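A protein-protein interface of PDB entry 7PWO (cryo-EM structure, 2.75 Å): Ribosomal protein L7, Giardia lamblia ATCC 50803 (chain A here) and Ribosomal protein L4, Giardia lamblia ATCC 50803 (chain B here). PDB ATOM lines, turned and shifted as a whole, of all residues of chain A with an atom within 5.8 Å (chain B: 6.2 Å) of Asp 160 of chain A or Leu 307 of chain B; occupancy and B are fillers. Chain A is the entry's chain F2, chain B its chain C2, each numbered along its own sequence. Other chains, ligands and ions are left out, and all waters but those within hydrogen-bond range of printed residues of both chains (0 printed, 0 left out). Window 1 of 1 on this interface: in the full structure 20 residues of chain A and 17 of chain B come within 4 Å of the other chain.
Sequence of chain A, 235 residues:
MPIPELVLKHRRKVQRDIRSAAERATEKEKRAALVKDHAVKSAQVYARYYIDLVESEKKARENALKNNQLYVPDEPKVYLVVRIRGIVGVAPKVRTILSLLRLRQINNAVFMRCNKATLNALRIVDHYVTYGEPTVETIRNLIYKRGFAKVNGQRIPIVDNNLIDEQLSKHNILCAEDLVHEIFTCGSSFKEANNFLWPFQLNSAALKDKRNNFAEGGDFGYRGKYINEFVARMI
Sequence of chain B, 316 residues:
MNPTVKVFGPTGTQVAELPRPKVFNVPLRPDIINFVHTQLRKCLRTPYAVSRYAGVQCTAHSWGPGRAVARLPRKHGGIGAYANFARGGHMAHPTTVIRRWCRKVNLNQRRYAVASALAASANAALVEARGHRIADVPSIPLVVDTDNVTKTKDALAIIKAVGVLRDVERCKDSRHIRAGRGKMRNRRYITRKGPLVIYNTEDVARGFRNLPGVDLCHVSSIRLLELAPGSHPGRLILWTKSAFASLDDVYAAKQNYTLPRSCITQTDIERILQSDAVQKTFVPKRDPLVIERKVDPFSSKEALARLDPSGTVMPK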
ATOM      1  N   ALA A  39      11.494  25.987  17.235  1.00  0.00           N
ATOM      2  CA  ALA A  39      10.042  26.011  17.111  1.00  0.00           C
ATOM      3  C   ALA A  39       9.377  25.502  18.378  1.00  0.00           C
ATOM      4  O   ALA A  39       8.440  26.120  18.895  1.00  0.00           O
ATOM      5  CB  ALA A  39       9.608  25.179  15.908  1.00  0.00           C
ATOM      6  N   TYR A 144      -2.995  30.157   9.727  1.00  0.00           N
ATOM      7  CA  TYR A 144      -2.875  28.725   9.490  1.00  0.00           C
ATOM      8  C   TYR A 144      -3.850  28.219   8.427  1.00  0.00           C
ATOM      9  O   TYR A 144      -3.506  27.298   7.685  1.00  0.00           O
ATOM     10  CB  TYR A 144      -3.080  27.962  10.799  1.00  0.00           C
ATOM     11  CG  TYR A 144      -1.922  28.018  11.786  1.00  0.00           C
ATOM     12  CD1 TYR A 144      -1.477  29.229  12.299  1.00  0.00           C
ATOM     13  CD2 TYR A 144      -1.323  26.857  12.253  1.00  0.00           C
ATOM     14  CE1 TYR A 144      -0.450  29.284  13.203  1.00  0.00           C
ATOM     15  CE2 TYR A 144      -0.296  26.904  13.165  1.00  0.00           C
ATOM     16  CZ  TYR A 144       0.136  28.123  13.642  1.00  0.00           C
ATOM     17  OH  TYR A 144       1.159  28.185  14.553  1.00  0.00           O
ATOM     18  N   PRO A 157       1.986  29.360  -1.114  1.00  0.00           N
ATOM     19  CA  PRO A 157       1.342  28.853   0.108  1.00  0.00           C
ATOM     20  C   PRO A 157       2.296  28.792   1.290  1.00  0.00           C
ATOM     21  O   PRO A 157       3.476  28.473   1.141  1.00  0.00           O
ATOM     22  CB  PRO A 157       0.876  27.454  -0.303  1.00  0.00           C
ATOM     23  CG  PRO A 157       0.647  27.560  -1.771  1.00  0.00           C
ATOM     24  CD  PRO A 157       1.604  28.587  -2.305  1.00  0.00           C
ATOM     25  N   ILE A 158       1.775  29.106   2.476  1.00  0.00           N
ATOM     26  CA  ILE A 158       2.506  28.984   3.734  1.00  0.00           C
ATOM     27  C   ILE A 158       2.070  27.653   4.337  1.00  0.00           C
ATOM     28  O   ILE A 158       0.985  27.542   4.907  1.00  0.00           O
ATOM     29  CB  ILE A 158       2.216  30.157   4.682  1.00  0.00           C
ATOM     30  CG1 ILE A 158       3.020  31.392   4.312  1.00  0.00           C
ATOM     31  CG2 ILE A 158       2.591  29.820   6.107  1.00  0.00           C
ATOM     32  CD1 ILE A 158       2.343  32.676   4.697  1.00  0.00           C
ATOM     33  N   VAL A 159       2.887  26.618   4.179  1.00  0.00           N
ATOM     34  CA  VAL A 159       2.537  25.304   4.699  1.00  0.00           C
ATOM     35  C   VAL A 159       3.542  24.766   5.708  1.00  0.00           C
ATOM     36  O   VAL A 159       3.198  23.840   6.457  1.00  0.00           O
ATOM     37  CB  VAL A 159       2.328  24.286   3.557  1.00  0.00           C
ATOM     38  CG1 VAL A 159       1.182  24.714   2.679  1.00  0.00           C
ATOM     39  CG2 VAL A 159       3.589  24.114   2.737  1.00  0.00           C
ATOM     40  N   ASP A 160       4.756  25.308   5.787  1.00  0.00           N
ATOM     41  CA  ASP A 160       5.750  24.820   6.732  1.00  0.00           C
ATOM     42  C   ASP A 160       6.623  25.975   7.202  1.00  0.00           C
ATOM     43  O   ASP A 160       6.524  27.098   6.706  1.00  0.00           O
ATOM     44  CB  ASP A 160       6.594  23.704   6.119  1.00  0.00           C
ATOM     45  CG  ASP A 160       7.486  24.182   5.007  1.00  0.00           C
ATOM     46  OD1 ASP A 160       7.221  25.259   4.433  1.00  0.00           O
ATOM     47  OD2 ASP A 160       8.447  23.460   4.688  1.00  0.00           O
ATOM     48  N   ASN A 161       7.482  25.684   8.176  1.00  0.00           N
ATOM     49  CA  ASN A 161       8.396  26.674   8.729  1.00  0.00           C
ATOM     50  C   ASN A 161       9.670  26.823   7.924  1.00  0.00           C
ATOM     51  O   ASN A 161      10.537  27.609   8.316  1.00  0.00           O
ATOM     52  CB  ASN A 161       8.774  26.331  10.169  1.00  0.00           C
ATOM     53  CG  ASN A 161       7.597  26.351  11.101  1.00  0.00           C
ATOM     54  OD1 ASN A 161       7.150  27.411  11.535  1.00  0.00           O
ATOM     55  ND2 ASN A 161       7.112  25.175  11.454  1.00  0.00           N
ATOM     56  N   ASN A 162       9.825  26.067   6.839  1.00  0.00           N
ATOM     57  CA  ASN A 162      10.996  26.232   5.992  1.00  0.00           C
ATOM     58  C   ASN A 162      10.971  27.566   5.258  1.00  0.00           C
ATOM     59  O   ASN A 162      12.025  28.161   5.019  1.00  0.00           O
ATOM     60  CB  ASN A 162      11.089  25.078   4.996  1.00  0.00           C
ATOM     61  CG  ASN A 162      11.331  23.734   5.671  1.00  0.00           C
ATOM     62  OD1 ASN A 162      12.048  23.641   6.667  1.00  0.00           O
ATOM     63  ND2 ASN A 162      10.736  22.685   5.122  1.00  0.00           N
ATOM     64  N   LEU A 163       9.787  28.056   4.905  1.00  0.00           N
ATOM     65  CA  LEU A 163       9.675  29.247   4.077  1.00  0.00           C
ATOM     66  C   LEU A 163       9.561  30.533   4.888  1.00  0.00           C
ATOM     67  O   LEU A 163       9.630  31.616   4.310  1.00  0.00           O
ATOM     68  CB  LEU A 163       8.477  29.100   3.132  1.00  0.00           C
ATOM     69  CG  LEU A 163       8.226  30.150   2.045  1.00  0.00           C
ATOM     70  CD1 LEU A 163       9.022  29.812   0.809  1.00  0.00           C
ATOM     71  CD2 LEU A 163       6.769  30.201   1.720  1.00  0.00           C
ATOM     72  N   ILE A 164       9.414  30.447   6.205  1.00  0.00           N
ATOM     73  CA  ILE A 164       9.452  31.647   7.030  1.00  0.00           C
ATOM     74  C   ILE A 164      10.869  31.961   7.502  1.00  0.00           C
ATOM     75  O   ILE A 164      11.258  33.131   7.557  1.00  0.00           O
ATOM     76  CB  ILE A 164       8.482  31.510   8.216  1.00  0.00           C
ATOM     77  CG1 ILE A 164       7.044  31.440   7.715  1.00  0.00           C
ATOM     78  CG2 ILE A 164       8.638  32.657   9.177  1.00  0.00           C
ATOM     79  CD1 ILE A 164       6.158  30.521   8.520  1.00  0.00           C
ATOM     80  N   CYS A 175       9.534  31.063  12.876  1.00  0.00           N
ATOM     81  CA  CYS A 175       8.480  30.065  12.906  1.00  0.00           C
ATOM     82  C   CYS A 175       7.122  30.733  12.756  1.00  0.00           C
ATOM     83  O   CYS A 175       6.976  31.956  12.868  1.00  0.00           O
ATOM     84  CB  CYS A 175       8.544  29.226  14.192  1.00  0.00           C
ATOM     85  SG  CYS A 175       7.971  30.069  15.681  1.00  0.00           S
ATOM     86  N   ALA A 176       6.119  29.895  12.490  1.00  0.00           N
ATOM     87  CA  ALA A 176       4.745  30.373  12.420  1.00  0.00           C
ATOM     88  C   ALA A 176       4.303  30.996  13.735  1.00  0.00           C
ATOM     89  O   ALA A 176       3.557  31.980  13.734  1.00  0.00           O
ATOM     90  CB  ALA A 176       3.816  29.226  12.025  1.00  0.00           C
ATOM     91  N   VAL B 290      10.597  25.770  -3.307  1.00  0.00           N
ATOM     92  CA  VAL B 290       9.812  24.545  -3.272  1.00  0.00           C
ATOM     93  C   VAL B 290       8.361  24.924  -2.984  1.00  0.00           C
ATOM     94  O   VAL B 290       8.063  25.587  -1.983  1.00  0.00           O
ATOM     95  CB  VAL B 290      10.389  23.529  -2.268  1.00  0.00           C
ATOM     96  CG1 VAL B 290      10.324  24.025  -0.831  1.00  0.00           C
ATOM     97  CG2 VAL B 290       9.676  22.191  -2.406  1.00  0.00           C
ATOM     98  N   GLU B 292       4.240  23.947  -2.801  1.00  0.00           N
ATOM     99  CA  GLU B 292       3.205  22.967  -2.546  1.00  0.00           C
ATOM    100  C   GLU B 292       1.844  23.609  -2.777  1.00  0.00           C
ATOM    101  O   GLU B 292       1.730  24.819  -2.973  1.00  0.00           O
ATOM    102  CB  GLU B 292       3.319  22.414  -1.122  1.00  0.00           C
ATOM    103  CG  GLU B 292       4.669  21.754  -0.838  1.00  0.00           C
ATOM    104  CD  GLU B 292       4.629  20.811   0.350  1.00  0.00           C
ATOM    105  OE1 GLU B 292       3.796  19.880   0.351  1.00  0.00           O
ATOM    106  OE2 GLU B 292       5.439  20.993   1.279  1.00  0.00           O
ATOM    107  N   PRO B 297      -3.874  22.640   7.553  1.00  0.00           N
ATOM    108  CA  PRO B 297      -3.068  21.904   8.544  1.00  0.00           C
ATOM    109  C   PRO B 297      -3.898  21.261   9.638  1.00  0.00           C
ATOM    110  O   PRO B 297      -3.613  20.134  10.055  1.00  0.00           O
ATOM    111  CB  PRO B 297      -2.130  22.981   9.111  1.00  0.00           C
ATOM    112  CG  PRO B 297      -2.650  24.259   8.673  1.00  0.00           C
ATOM    113  CD  PRO B 297      -3.458  24.046   7.443  1.00  0.00           C
ATOM    114  N   GLU B 302      -0.170  15.206  11.395  1.00  0.00           N
ATOM    115  CA  GLU B 302       1.101  15.419  10.709  1.00  0.00           C
ATOM    116  C   GLU B 302       1.102  16.722   9.910  1.00  0.00           C
ATOM    117  O   GLU B 302       2.115  17.437   9.874  1.00  0.00           O
ATOM    118  CB  GLU B 302       1.438  14.207   9.836  1.00  0.00           C
ATOM    119  CG  GLU B 302       0.550  13.969   8.624  1.00  0.00           C
ATOM    120  CD  GLU B 302      -0.706  13.170   8.964  1.00  0.00           C
ATOM    121  OE1 GLU B 302      -1.039  13.055  10.162  1.00  0.00           O
ATOM    122  OE2 GLU B 302      -1.354  12.644   8.034  1.00  0.00           O
ATOM    123  N   ALA B 303      -0.031  17.062   9.289  1.00  0.00           N
ATOM    124  CA  ALA B 303      -0.124  18.320   8.558  1.00  0.00           C
ATOM    125  C   ALA B 303       0.091  19.513   9.484  1.00  0.00           C
ATOM    126  O   ALA B 303       0.772  20.474   9.116  1.00  0.00           O
ATOM    127  CB  ALA B 303      -1.472  18.414   7.845  1.00  0.00           C
ATOM    128  N   LEU B 304      -0.474  19.466  10.695  1.00  0.00           N
ATOM    129  CA  LEU B 304      -0.244  20.528  11.675  1.00  0.00           C
ATOM    130  C   LEU B 304       1.177  20.494  12.224  1.00  0.00           C
ATOM    131  O   LEU B 304       1.785  21.545  12.472  1.00  0.00           O
ATOM    132  CB  LEU B 304      -1.246  20.408  12.824  1.00  0.00           C
ATOM    133  CG  LEU B 304      -1.585  21.695  13.588  1.00  0.00           C
ATOM    134  CD1 LEU B 304      -1.797  22.886  12.665  1.00  0.00           C
ATOM    135  CD2 LEU B 304      -2.783  21.473  14.469  1.00  0.00           C
ATOM    136  N   ALA B 305       1.712  19.293  12.442  1.00  0.00           N
ATOM    137  CA  ALA B 305       3.033  19.138  13.028  1.00  0.00           C
ATOM    138  C   ALA B 305       4.141  19.528  12.068  1.00  0.00           C
ATOM    139  O   ALA B 305       5.301  19.613  12.485  1.00  0.00           O
ATOM    140  CB  ALA B 305       3.239  17.700  13.502  1.00  0.00           C
ATOM    141  N   ARG B 306       3.820  19.739  10.793  1.00  0.00           N
ATOM    142  CA  ARG B 306       4.780  20.409   9.927  1.00  0.00           C
ATOM    143  C   ARG B 306       5.031  21.844  10.393  1.00  0.00           C
ATOM    144  O   ARG B 306       6.183  22.292  10.437  1.00  0.00           O
ATOM    145  CB  ARG B 306       4.302  20.376   8.483  1.00  0.00           C
ATOM    146  CG  ARG B 306       5.324  20.921   7.537  1.00  0.00           C
ATOM    147  CD  ARG B 306       5.198  20.343   6.158  1.00  0.00           C
ATOM    148  NE  ARG B 306       6.430  20.512   5.400  1.00  0.00           N
ATOM    149  CZ  ARG B 306       6.535  20.278   4.098  1.00  0.00           C
ATOM    150  NH1 ARG B 306       7.696  20.447   3.483  1.00  0.00           N
ATOM    151  NH2 ARG B 306       5.473  19.869   3.416  1.00  0.00           N
ATOM    152  N   LEU B 307       3.972  22.571  10.776  1.00  0.00           N
ATOM    153  CA  LEU B 307       4.146  23.927  11.308  1.00  0.00           C
ATOM    154  C   LEU B 307       4.610  23.934  12.763  1.00  0.00           C
ATOM    155  O   LEU B 307       5.713  24.399  13.067  1.00  0.00           O
ATOM    156  CB  LEU B 307       2.858  24.744  11.167  1.00  0.00           C
ATOM    157  CG  LEU B 307       2.544  25.470   9.854  1.00  0.00           C
ATOM    158  CD1 LEU B 307       1.439  26.445  10.088  1.00  0.00           C
ATOM    159  CD2 LEU B 307       3.756  26.226   9.384  1.00  0.00           C
ATOM    160  N   ASP B 308       3.798  23.424  13.684  1.00  0.00           N
ATOM    161  CA  ASP B 308       4.215  23.454  15.090  1.00  0.00           C
ATOM    162  C   ASP B 308       4.315  22.056  15.683  1.00  0.00           C
ATOM    163  O   ASP B 308       3.277  21.407  15.916  1.00  0.00           O
ATOM    164  CB  ASP B 308       3.296  24.321  15.945  1.00  0.00           C
ATOM    165  CG  ASP B 308       3.933  24.667  17.290  1.00  0.00           C
ATOM    166  OD1 ASP B 308       5.012  25.299  17.288  1.00  0.00           O
ATOM    167  OD2 ASP B 308       3.371  24.292  18.341  1.00  0.00           O
ATOM    168  N   PRO B 309       5.527  21.569  15.952  1.00  0.00           N
ATOM    169  CA  PRO B 309       5.705  20.186  16.428  1.00  0.00           C
ATOM    170  C   PRO B 309       5.447  19.990  17.915  1.00  0.00           C
ATOM    171  O   PRO B 309       5.013  18.911  18.334  1.00  0.00           O
ATOM    172  CB  PRO B 309       7.174  19.887  16.088  1.00  0.00           C
ATOM    173  CG  PRO B 309       7.641  21.040  15.210  1.00  0.00           C
ATOM    174  CD  PRO B 309       6.800  22.208  15.591  1.00  0.00           C
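ND2 of Asn 161 of chain A sits at hydrogen-bond distance from O of Arg 306 of chain B (3.2 Å).
OD2 of Asp 160 of chain A lies within salt-bridge range of NH1 of Arg 306 of chain B, at 3.3 Å.
O of Leu 307 of chain B sits close to ND2 of Asn 161 of chain A (2.3 Å).
The backbone NH (N) of Leu 304 of chain B sits at hydrogen-bond distance from the backbone carbonyl oxygen (O) of Pro 297 of chain B, 3.3 Å away.
The side-chain carboxylate (OE2) of Glu 292 of chain B is in salt-bridge range of the guanidinium group (NH2) of Arg 306 of chain B (2.4 Å).
OD2 of Asp 160 of chain A sits at hydrogen-bond distance from ND2 of Asn 162 of chain A (2.5 Å).
N of Ala 176 of chain A sits at hydrogen-bond distance from OD1 of Asn 161 of chain A (2.9 Å).
O of Ala 39 of chain A touches OD1 of Asp 308 of chain B, 3.9 Å away.
Tyr 144 of chain A touches Pro 297 of chain B (O to CD, 3.3 Å).
Tyr 144 of chain A touches Leu 307 of chain B.
O of Glu 292 of chain B touches CG of Pro 157 of chain A (3.2 Å).
CG2 of Val 159 of chain A touches OE2 of Glu 292 of chain B, at 3.9 Å.
Val 159 of chain A touches Arg 306 of chain B (O to CG, 3.8 Å).
Leu 307 of chain B touches Val 159 of chain A.
CA of Asp 160 of chain A touches CD2 of Leu 307 of chain B (3.6 Å).
Ala 176 of chain A touches Leu 307 of chain B.
Of chain B, only Arg 306 (3.3 Å) and Leu 307 (3.6 Å) come within 4 Å of Asp 160 of chain A.
Of the printed residues of chain A, Leu 307 of chain B touches Tyr 144 (3.5 Å), Val 159 (3.8 Å), Asp 160 (3.6 Å), Asn 161 (2.3 Å) and Ala 176 (3.997 Å).
Of the printed residues of chain B, Ala 176 of chain A touches Leu 307 (3.997 Å).
Of the printed residues of chain A, Pro 297 of chain B touches Tyr 144.
Printed residues of chain B within 4 Å of Tyr 144 of chain A: Pro 297 and Leu 307.
Printed residues of chain A within 4 Å of Asp 308 of chain B: Ala 39 (3.9 Å).
Asn 162 of chain A touches none of the printed residues of chain B.
Cys 175 of chain A touches none of the printed residues of chain B.
The nearest residue of chain B that does not touch Asp 160 of chain A is Glu 292 of chain B (5.2 Å).
Of the 11 printed residues of chain B, 5 touch a printed residue of chain A.
Hydrophobic or aromatic side chains of chain A within 4 Å of the printed part of chain B: Tyr 144, Pro 157, Val 159 and Ala 176.
Among the printed residues, Asp or Glu carboxylates within 4 Å of a Lys or Arg side-chain nitrogen of the other chain: Asp 160 of chain A with Arg 306 of chain B.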
